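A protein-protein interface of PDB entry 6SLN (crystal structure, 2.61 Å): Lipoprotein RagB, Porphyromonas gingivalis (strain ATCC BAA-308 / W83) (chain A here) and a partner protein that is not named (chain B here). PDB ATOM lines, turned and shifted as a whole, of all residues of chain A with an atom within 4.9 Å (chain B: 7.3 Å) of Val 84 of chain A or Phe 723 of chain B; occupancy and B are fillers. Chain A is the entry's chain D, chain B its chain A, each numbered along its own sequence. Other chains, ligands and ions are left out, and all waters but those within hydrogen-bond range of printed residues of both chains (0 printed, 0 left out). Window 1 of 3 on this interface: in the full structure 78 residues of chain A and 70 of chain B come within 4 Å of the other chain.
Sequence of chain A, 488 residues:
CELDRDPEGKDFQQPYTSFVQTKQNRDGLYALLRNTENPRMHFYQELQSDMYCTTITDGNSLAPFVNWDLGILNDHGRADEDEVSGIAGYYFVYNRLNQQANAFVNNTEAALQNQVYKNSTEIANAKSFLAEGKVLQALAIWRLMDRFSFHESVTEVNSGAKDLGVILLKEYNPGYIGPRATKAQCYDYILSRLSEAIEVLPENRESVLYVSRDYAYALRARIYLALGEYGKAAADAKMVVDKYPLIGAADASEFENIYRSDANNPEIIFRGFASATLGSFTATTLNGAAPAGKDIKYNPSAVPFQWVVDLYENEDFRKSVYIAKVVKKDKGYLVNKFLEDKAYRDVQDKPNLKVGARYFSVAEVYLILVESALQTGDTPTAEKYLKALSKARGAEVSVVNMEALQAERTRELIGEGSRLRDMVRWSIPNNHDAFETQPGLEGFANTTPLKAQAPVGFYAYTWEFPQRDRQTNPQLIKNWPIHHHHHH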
ATOM      1  N   MET A  41      25.838  21.618   5.402  1.00  0.00           N
ATOM      2  CA  MET A  41      24.462  21.381   5.803  1.00  0.00           C
ATOM      3  C   MET A  41      23.531  21.246   4.608  1.00  0.00           C
ATOM      4  O   MET A  41      22.472  20.634   4.746  1.00  0.00           O
ATOM      5  CB  MET A  41      23.990  22.502   6.741  1.00  0.00           C
ATOM      6  CG  MET A  41      24.311  22.248   8.218  1.00  0.00           C
ATOM      7  SD  MET A  41      23.717  20.612   8.696  1.00  0.00           S
ATOM      8  CE  MET A  41      24.234  20.522  10.407  1.00  0.00           C
ATOM      9  N   ARG A  78      21.472  13.093  12.887  1.00  0.00           N
ATOM     10  CA  ARG A  78      21.753  13.105  14.312  1.00  0.00           C
ATOM     11  C   ARG A  78      21.901  14.544  14.768  1.00  0.00           C
ATOM     12  O   ARG A  78      22.194  15.449  13.971  1.00  0.00           O
ATOM     13  CB  ARG A  78      23.025  12.329  14.646  1.00  0.00           C
ATOM     14  CG  ARG A  78      22.909  10.860  14.367  1.00  0.00           C
ATOM     15  CD  ARG A  78      23.412  10.065  15.524  1.00  0.00           C
ATOM     16  NE  ARG A  78      24.776  10.447  15.842  1.00  0.00           N
ATOM     17  CZ  ARG A  78      25.299  10.344  17.053  1.00  0.00           C
ATOM     18  NH1 ARG A  78      24.559   9.878  18.054  1.00  0.00           N
ATOM     19  NH2 ARG A  78      26.554  10.714  17.264  1.00  0.00           N
ATOM     20  N   ALA A  79      21.707  14.737  16.080  1.00  0.00           N
ATOM     21  CA  ALA A  79      21.901  16.043  16.729  1.00  0.00           C
ATOM     22  C   ALA A  79      22.049  15.752  18.218  1.00  0.00           C
ATOM     23  O   ALA A  79      21.046  15.597  18.929  1.00  0.00           O
ATOM     24  CB  ALA A  79      20.751  17.006  16.461  1.00  0.00           C
ATOM     25  N   ASP A  80      23.296  15.654  18.663  1.00  0.00           N
ATOM     26  CA  ASP A  80      23.614  15.398  20.051  1.00  0.00           C
ATOM     27  C   ASP A  80      24.990  16.000  20.301  1.00  0.00           C
ATOM     28  O   ASP A  80      25.551  16.668  19.427  1.00  0.00           O
ATOM     29  CB  ASP A  80      23.546  13.895  20.347  1.00  0.00           C
ATOM     30  CG  ASP A  80      24.425  13.072  19.410  1.00  0.00           C
ATOM     31  OD1 ASP A  80      25.460  13.585  18.909  1.00  0.00           O
ATOM     32  OD2 ASP A  80      24.080  11.900  19.185  1.00  0.00           O
ATOM     33  N   GLU A  81      25.550  15.737  21.485  1.00  0.00           N
ATOM     34  CA  GLU A  81      26.883  16.244  21.793  1.00  0.00           C
ATOM     35  C   GLU A  81      27.960  15.637  20.906  1.00  0.00           C
ATOM     36  O   GLU A  81      28.993  16.268  20.673  1.00  0.00           O
ATOM     37  CB  GLU A  81      27.245  15.985  23.259  1.00  0.00           C
ATOM     38  CG  GLU A  81      27.004  17.153  24.217  1.00  0.00           C
ATOM     39  CD  GLU A  81      27.505  18.530  23.725  1.00  0.00           C
ATOM     40  OE1 GLU A  81      27.097  19.546  24.352  1.00  0.00           O
ATOM     41  OE2 GLU A  81      28.310  18.624  22.771  1.00  0.00           O
ATOM     42  N   ASP A  82      27.764  14.434  20.404  1.00  0.00           N
ATOM     43  CA  ASP A  82      28.855  13.854  19.641  1.00  0.00           C
ATOM     44  C   ASP A  82      28.836  14.260  18.175  1.00  0.00           C
ATOM     45  O   ASP A  82      29.905  14.444  17.587  1.00  0.00           O
ATOM     46  CB  ASP A  82      28.825  12.338  19.780  1.00  0.00           C
ATOM     47  CG  ASP A  82      28.984  11.897  21.222  1.00  0.00           C
ATOM     48  OD1 ASP A  82      29.803  12.511  21.939  1.00  0.00           O
ATOM     49  OD2 ASP A  82      28.279  10.954  21.644  1.00  0.00           O
ATOM     50  N   GLU A  83      27.659  14.454  17.585  1.00  0.00           N
ATOM     51  CA  GLU A  83      27.565  14.694  16.153  1.00  0.00           C
ATOM     52  C   GLU A  83      26.262  15.430  15.871  1.00  0.00           C
ATOM     53  O   GLU A  83      25.233  15.113  16.466  1.00  0.00           O
ATOM     54  CB  GLU A  83      27.625  13.354  15.389  1.00  0.00           C
ATOM     55  CG  GLU A  83      28.087  13.418  13.931  1.00  0.00           C
ATOM     56  CD  GLU A  83      27.565  12.245  13.102  1.00  0.00           C
ATOM     57  OE1 GLU A  83      26.871  11.374  13.669  1.00  0.00           O
ATOM     58  OE2 GLU A  83      27.852  12.194  11.886  1.00  0.00           O
ATOM     59  N   VAL A  84      26.314  16.400  14.960  1.00  0.00           N
ATOM     60  CA  VAL A  84      25.139  17.104  14.453  1.00  0.00           C
ATOM     61  C   VAL A  84      25.240  17.021  12.934  1.00  0.00           C
ATOM     62  O   VAL A  84      26.038  17.735  12.318  1.00  0.00           O
ATOM     63  CB  VAL A  84      25.058  18.563  14.943  1.00  0.00           C
ATOM     64  CG1 VAL A  84      24.137  19.414  14.062  1.00  0.00           C
ATOM     65  CG2 VAL A  84      24.574  18.608  16.396  1.00  0.00           C
ATOM     66  N   SER A  85      24.446  16.138  12.326  1.00  0.00           N
ATOM     67  CA  SER A  85      24.540  15.878  10.892  1.00  0.00           C
ATOM     68  C   SER A  85      23.184  15.458  10.342  1.00  0.00           C
ATOM     69  O   SER A  85      22.279  15.045  11.073  1.00  0.00           O
ATOM     70  CB  SER A  85      25.574  14.789  10.578  1.00  0.00           C
ATOM     71  OG  SER A  85      25.343  13.613  11.354  1.00  0.00           O
ATOM     72  N   GLY A  86      23.059  15.563   9.043  1.00  0.00           N
ATOM     73  CA  GLY A  86      21.913  14.986   8.390  1.00  0.00           C
ATOM     74  C   GLY A  86      20.638  15.782   8.594  1.00  0.00           C
ATOM     75  O   GLY A  86      20.633  16.959   8.982  1.00  0.00           O
ATOM     76  N   GLY A  89      20.190  16.975  11.963  1.00  0.00           N
ATOM     77  CA  GLY A  89      21.147  18.045  12.205  1.00  0.00           C
ATOM     78  C   GLY A  89      20.765  19.351  11.528  1.00  0.00           C
ATOM     79  O   GLY A  89      20.804  20.421  12.149  1.00  0.00           O
ATOM     80  N   PHE A  92      18.051  20.747  13.523  1.00  0.00           N
ATOM     81  CA  PHE A  92      18.487  21.273  14.813  1.00  0.00           C
ATOM     82  C   PHE A  92      19.231  22.603  14.674  1.00  0.00           C
ATOM     83  O   PHE A  92      18.891  23.573  15.357  1.00  0.00           O
ATOM     84  CB  PHE A  92      19.361  20.250  15.531  1.00  0.00           C
ATOM     85  CG  PHE A  92      20.071  20.803  16.724  1.00  0.00           C
ATOM     86  CD1 PHE A  92      19.413  20.930  17.935  1.00  0.00           C
ATOM     87  CD2 PHE A  92      21.383  21.215  16.636  1.00  0.00           C
ATOM     88  CE1 PHE A  92      20.056  21.434  19.047  1.00  0.00           C
ATOM     89  CE2 PHE A  92      22.038  21.734  17.745  1.00  0.00           C
ATOM     90  CZ  PHE A  92      21.371  21.848  18.953  1.00  0.00           C
ATOM     91  N   VAL A  93      20.272  22.669  13.832  1.00  0.00           N
ATOM     92  CA  VAL A  93      21.083  23.889  13.806  1.00  0.00           C
ATOM     93  C   VAL A  93      20.238  25.105  13.437  1.00  0.00           C
ATOM     94  O   VAL A  93      20.436  26.196  13.982  1.00  0.00           O
ATOM     95  CB  VAL A  93      22.301  23.751  12.871  1.00  0.00           C
ATOM     96  CG1 VAL A  93      23.155  22.634  13.325  1.00  0.00           C
ATOM     97  CG2 VAL A  93      21.877  23.559  11.419  1.00  0.00           C
ATOM     98  N   ARG A 468      12.987  12.955  17.113  1.00  0.00           N
ATOM     99  CA  ARG A 468      13.064  13.573  18.424  1.00  0.00           C
ATOM    100  C   ARG A 468      11.886  14.503  18.642  1.00  0.00           C
ATOM    101  O   ARG A 468      11.200  14.416  19.660  1.00  0.00           O
ATOM    102  CB  ARG A 468      14.380  14.325  18.586  1.00  0.00           C
ATOM    103  CG  ARG A 468      14.414  15.221  19.826  1.00  0.00           C
ATOM    104  CD  ARG A 468      14.543  14.400  21.097  1.00  0.00           C
ATOM    105  NE  ARG A 468      15.901  13.907  21.255  1.00  0.00           N
ATOM    106  CZ  ARG A 468      16.904  14.621  21.749  1.00  0.00           C
ATOM    107  NH1 ARG A 468      16.705  15.873  22.155  1.00  0.00           N
ATOM    108  NH2 ARG A 468      18.107  14.072  21.842  1.00  0.00           N
ATOM    109  N   SER B 668      24.789  28.657  26.282  1.00  0.00           N
ATOM    110  CA  SER B 668      25.210  27.264  26.253  1.00  0.00           C
ATOM    111  C   SER B 668      24.200  26.322  26.891  1.00  0.00           C
ATOM    112  O   SER B 668      23.940  25.262  26.338  1.00  0.00           O
ATOM    113  CB  SER B 668      26.593  27.096  26.901  1.00  0.00           C
ATOM    114  OG  SER B 668      26.528  26.761  28.270  1.00  0.00           O
ATOM    115  N   ASP B 713      17.548  13.100  32.140  1.00  0.00           N
ATOM    116  CA  ASP B 713      18.225  13.977  31.193  1.00  0.00           C
ATOM    117  C   ASP B 713      17.227  14.155  30.049  1.00  0.00           C
ATOM    118  O   ASP B 713      17.245  13.446  29.035  1.00  0.00           O
ATOM    119  CB  ASP B 713      19.554  13.369  30.750  1.00  0.00           C
ATOM    120  CG  ASP B 713      20.473  14.373  30.092  1.00  0.00           C
ATOM    121  OD1 ASP B 713      20.045  15.522  29.876  1.00  0.00           O
ATOM    122  OD2 ASP B 713      21.628  14.014  29.784  1.00  0.00           O
ATOM    123  N   VAL B 714      16.313  15.098  30.245  1.00  0.00           N
ATOM    124  CA  VAL B 714      15.114  15.161  29.403  1.00  0.00           C
ATOM    125  C   VAL B 714      15.518  15.491  27.970  1.00  0.00           C
ATOM    126  O   VAL B 714      16.281  16.450  27.746  1.00  0.00           O
ATOM    127  CB  VAL B 714      14.125  16.191  29.955  1.00  0.00           C
ATOM    128  CG1 VAL B 714      13.119  16.564  28.889  1.00  0.00           C
ATOM    129  CG2 VAL B 714      13.410  15.642  31.207  1.00  0.00           C
ATOM    130  N   PRO B 715      15.078  14.706  26.985  1.00  0.00           N
ATOM    131  CA  PRO B 715      15.389  15.021  25.582  1.00  0.00           C
ATOM    132  C   PRO B 715      14.655  16.284  25.146  1.00  0.00           C
ATOM    133  O   PRO B 715      13.438  16.395  25.299  1.00  0.00           O
ATOM    134  CB  PRO B 715      14.891  13.782  24.814  1.00  0.00           C
ATOM    135  CG  PRO B 715      14.607  12.712  25.857  1.00  0.00           C
ATOM    136  CD  PRO B 715      14.299  13.461  27.124  1.00  0.00           C
ATOM    137  N   MET B 716      15.372  17.205  24.608  1.00  0.00           N
ATOM    138  CA  MET B 716      14.529  18.348  24.274  1.00  0.00           C
ATOM    139  C   MET B 716      14.131  18.317  22.804  1.00  0.00           C
ATOM    140  O   MET B 716      14.892  17.825  21.964  1.00  0.00           O
ATOM    141  CB  MET B 716      15.250  19.668  24.569  1.00  0.00           C
ATOM    142  CG  MET B 716      15.961  19.707  25.916  1.00  0.00           C
ATOM    143  SD  MET B 716      14.932  20.530  27.134  1.00  0.00           S
ATOM    144  CE  MET B 716      14.824  22.138  26.360  1.00  0.00           C
ATOM    145  N   PRO B 717      12.936  18.807  22.473  1.00  0.00           N
ATOM    146  CA  PRO B 717      12.614  19.062  21.065  1.00  0.00           C
ATOM    147  C   PRO B 717      13.619  20.023  20.463  1.00  0.00           C
ATOM    148  O   PRO B 717      14.010  21.008  21.090  1.00  0.00           O
ATOM    149  CB  PRO B 717      11.213  19.687  21.116  1.00  0.00           C
ATOM    150  CG  PRO B 717      10.908  19.922  22.562  1.00  0.00           C
ATOM    151  CD  PRO B 717      11.764  18.993  23.350  1.00  0.00           C
ATOM    152  N   TYR B 718      14.029  19.737  19.230  1.00  0.00           N
ATOM    153  CA  TYR B 718      15.092  20.505  18.600  1.00  0.00           C
ATOM    154  C   TYR B 718      14.674  21.929  18.270  1.00  0.00           C
ATOM    155  O   TYR B 718      15.545  22.754  17.989  1.00  0.00           O
ATOM    156  CB  TYR B 718      15.574  19.789  17.342  1.00  0.00           C
ATOM    157  CG  TYR B 718      16.355  18.538  17.641  1.00  0.00           C
ATOM    158  CD1 TYR B 718      17.152  18.447  18.773  1.00  0.00           C
ATOM    159  CD2 TYR B 718      16.284  17.428  16.799  1.00  0.00           C
ATOM    160  CE1 TYR B 718      17.875  17.290  19.049  1.00  0.00           C
ATOM    161  CE2 TYR B 718      16.999  16.277  17.073  1.00  0.00           C
ATOM    162  CZ  TYR B 718      17.794  16.213  18.192  1.00  0.00           C
ATOM    163  OH  TYR B 718      18.504  15.071  18.460  1.00  0.00           O
ATOM    164  N   SER B 720      13.912  23.773  20.491  1.00  0.00           N
ATOM    165  CA  SER B 720      14.507  24.417  21.660  1.00  0.00           C
ATOM    166  C   SER B 720      15.950  24.844  21.435  1.00  0.00           C
ATOM    167  O   SER B 720      16.442  25.707  22.171  1.00  0.00           O
ATOM    168  CB  SER B 720      14.473  23.473  22.864  1.00  0.00           C
ATOM    169  OG  SER B 720      15.620  22.620  22.871  1.00  0.00           O
ATOM    170  N   GLY B 721      16.654  24.236  20.473  1.00  0.00           N
ATOM    171  CA  GLY B 721      18.041  24.579  20.238  1.00  0.00           C
ATOM    172  C   GLY B 721      18.985  24.016  21.268  1.00  0.00           C
ATOM    173  O   GLY B 721      20.106  24.506  21.391  1.00  0.00           O
ATOM    174  N   PHE B 722      18.545  23.014  22.022  1.00  0.00           N
ATOM    175  CA  PHE B 722      19.341  22.314  23.012  1.00  0.00           C
ATOM    176  C   PHE B 722      19.138  20.823  22.815  1.00  0.00           C
ATOM    177  O   PHE B 722      18.105  20.396  22.291  1.00  0.00           O
ATOM    178  CB  PHE B 722      18.938  22.673  24.437  1.00  0.00           C
ATOM    179  CG  PHE B 722      19.110  24.118  24.769  1.00  0.00           C
ATOM    180  CD1 PHE B 722      20.340  24.605  25.185  1.00  0.00           C
ATOM    181  CD2 PHE B 722      18.042  24.993  24.665  1.00  0.00           C
ATOM    182  CE1 PHE B 722      20.505  25.930  25.488  1.00  0.00           C
ATOM    183  CE2 PHE B 722      18.214  26.324  24.969  1.00  0.00           C
ATOM    184  CZ  PHE B 722      19.447  26.787  25.387  1.00  0.00           C
ATOM    185  N   PHE B 723      20.129  20.034  23.249  1.00  0.00           N
ATOM    186  CA  PHE B 723      20.051  18.584  23.116  1.00  0.00           C
ATOM    187  C   PHE B 723      19.250  17.973  24.250  1.00  0.00           C
ATOM    188  O   PHE B 723      18.426  17.075  24.037  1.00  0.00           O
ATOM    189  CB  PHE B 723      21.443  17.963  23.110  1.00  0.00           C
ATOM    190  CG  PHE B 723      22.320  18.446  22.007  1.00  0.00           C
ATOM    191  CD1 PHE B 723      21.829  18.573  20.720  1.00  0.00           C
ATOM    192  CD2 PHE B 723      23.646  18.763  22.254  1.00  0.00           C
ATOM    193  CE1 PHE B 723      22.647  19.002  19.699  1.00  0.00           C
ATOM    194  CE2 PHE B 723      24.455  19.204  21.242  1.00  0.00           C
ATOM    195  CZ  PHE B 723      23.954  19.323  19.959  1.00  0.00           C
ATOM    196  N   SER B 724      19.504  18.434  25.465  1.00  0.00           N
ATOM    197  CA  SER B 724      18.927  17.814  26.643  1.00  0.00           C
ATOM    198  C   SER B 724      18.960  18.852  27.748  1.00  0.00           C
ATOM    199  O   SER B 724      19.535  19.932  27.590  1.00  0.00           O
ATOM    200  CB  SER B 724      19.682  16.527  27.015  1.00  0.00           C
ATOM    201  OG  SER B 724      20.658  16.749  28.019  1.00  0.00           O
ATOM    202  N   GLN B 725      18.298  18.532  28.853  1.00  0.00           N
ATOM    203  CA  GLN B 725      18.347  19.368  30.047  1.00  0.00           C
ATOM    204  C   GLN B 725      17.802  18.535  31.185  1.00  0.00           C
ATOM    205  O   GLN B 725      16.671  18.036  31.100  1.00  0.00           O
ATOM    206  CB  GLN B 725      17.542  20.648  29.889  1.00  0.00           C
ATOM    207  CG  GLN B 725      17.381  21.429  31.204  1.00  0.00           C
ATOM    208  CD  GLN B 725      18.704  21.903  31.780  1.00  0.00           C
ATOM    209  OE1 GLN B 725      19.495  22.556  31.100  1.00  0.00           O
ATOM    210  NE2 GLN B 725      18.951  21.565  33.032  1.00  0.00           N
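OH of Tyr 718 of chain B lies within hydrogen-bond range of O of Ala 79 of chain A, 2.6 Å away. The backbone carbonyl oxygen (O) of Met 716 of chain B sits at hydrogen-bond distance from the guanidinium group (NH1) of Arg 468 of chain A. O of Phe 723 of chain B is in hydrogen-bond range of NH1 of Arg 468 of chain A, at 2.8 Å.
OG of Ser 720 of chain B is in hydrogen-bond range of N of Phe 722 of chain B (3.1 Å). The side-chain carboxylate (OD1) of Asp 80 of chain A lies within hydrogen-bond range of the backbone NH (N) of Asp 82 of chain A (2.9 Å). N of Met 716 of chain B sits at hydrogen-bond distance from O of Phe 723 of chain B, at 3.1 Å. NH2 of Arg 78 of chain A lies within salt-bridge range of OD2 of Asp 80 of chain A. The backbone NH (N) of Glu 83 of chain A sits at hydrogen-bond distance from the side-chain carboxylate (OD1) of Asp 80 of chain A (2.7 Å).
Among the printed residues, merely in contact across the chains: Asp 80 of chain A with Phe 723 of chain B, Phe 92 of chain A with Phe 723 of chain B, Phe 92 of chain A with Tyr 718 of chain B, Arg 468 of chain A with Tyr 718 of chain B, Ala 79 of chain A with Phe 723 of chain B, Phe 92 of chain A with Gly 721 of chain B, Glu 81 of chain A with Phe 723 of chain B, Arg 468 of chain A with Pro 715 of chain B, Val 84 of chain A with Phe 723 of chain B and Phe 92 of chain A with Phe 722 of chain B.
Printed residues of chain B within 4 Å of Arg 468 of chain A: Pro 715, Met 716, Tyr 718 and Phe 723. Of the printed residues of chain B, Asp 80 of chain A touches Phe 723 (3.1 Å). Printed residues of chain A within 4 Å of Pro 715 of chain B: Arg 468. Of the printed residues of chain A, Gly 721 of chain B touches Phe 92. The nearest printed residue of chain A that does not touch Gly 721 of chain B is Val 93 of chain A (6.9 Å).
Of the 14 printed residues of chain A, 6 touch a printed residue of chain B. Hydrophobic or aromatic side chains of chain A within 4 Å of the printed part of chain B: Ala 79, Val 84 and Phe 92. Of the 13 printed residues of chain B, 6 touch a printed residue of chain A. Printed residues of chain B that touch a printed residue of chain A: Pro 715, Met 716, Tyr 718, Gly 721, Phe 722 and Phe 723. Among the printed residues, 13 pairs touch across the chains. Among the printed residues, no Asp or Glu carboxylate lies within 4 Å of a Lys or Arg side-chain nitrogen of the other chain.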
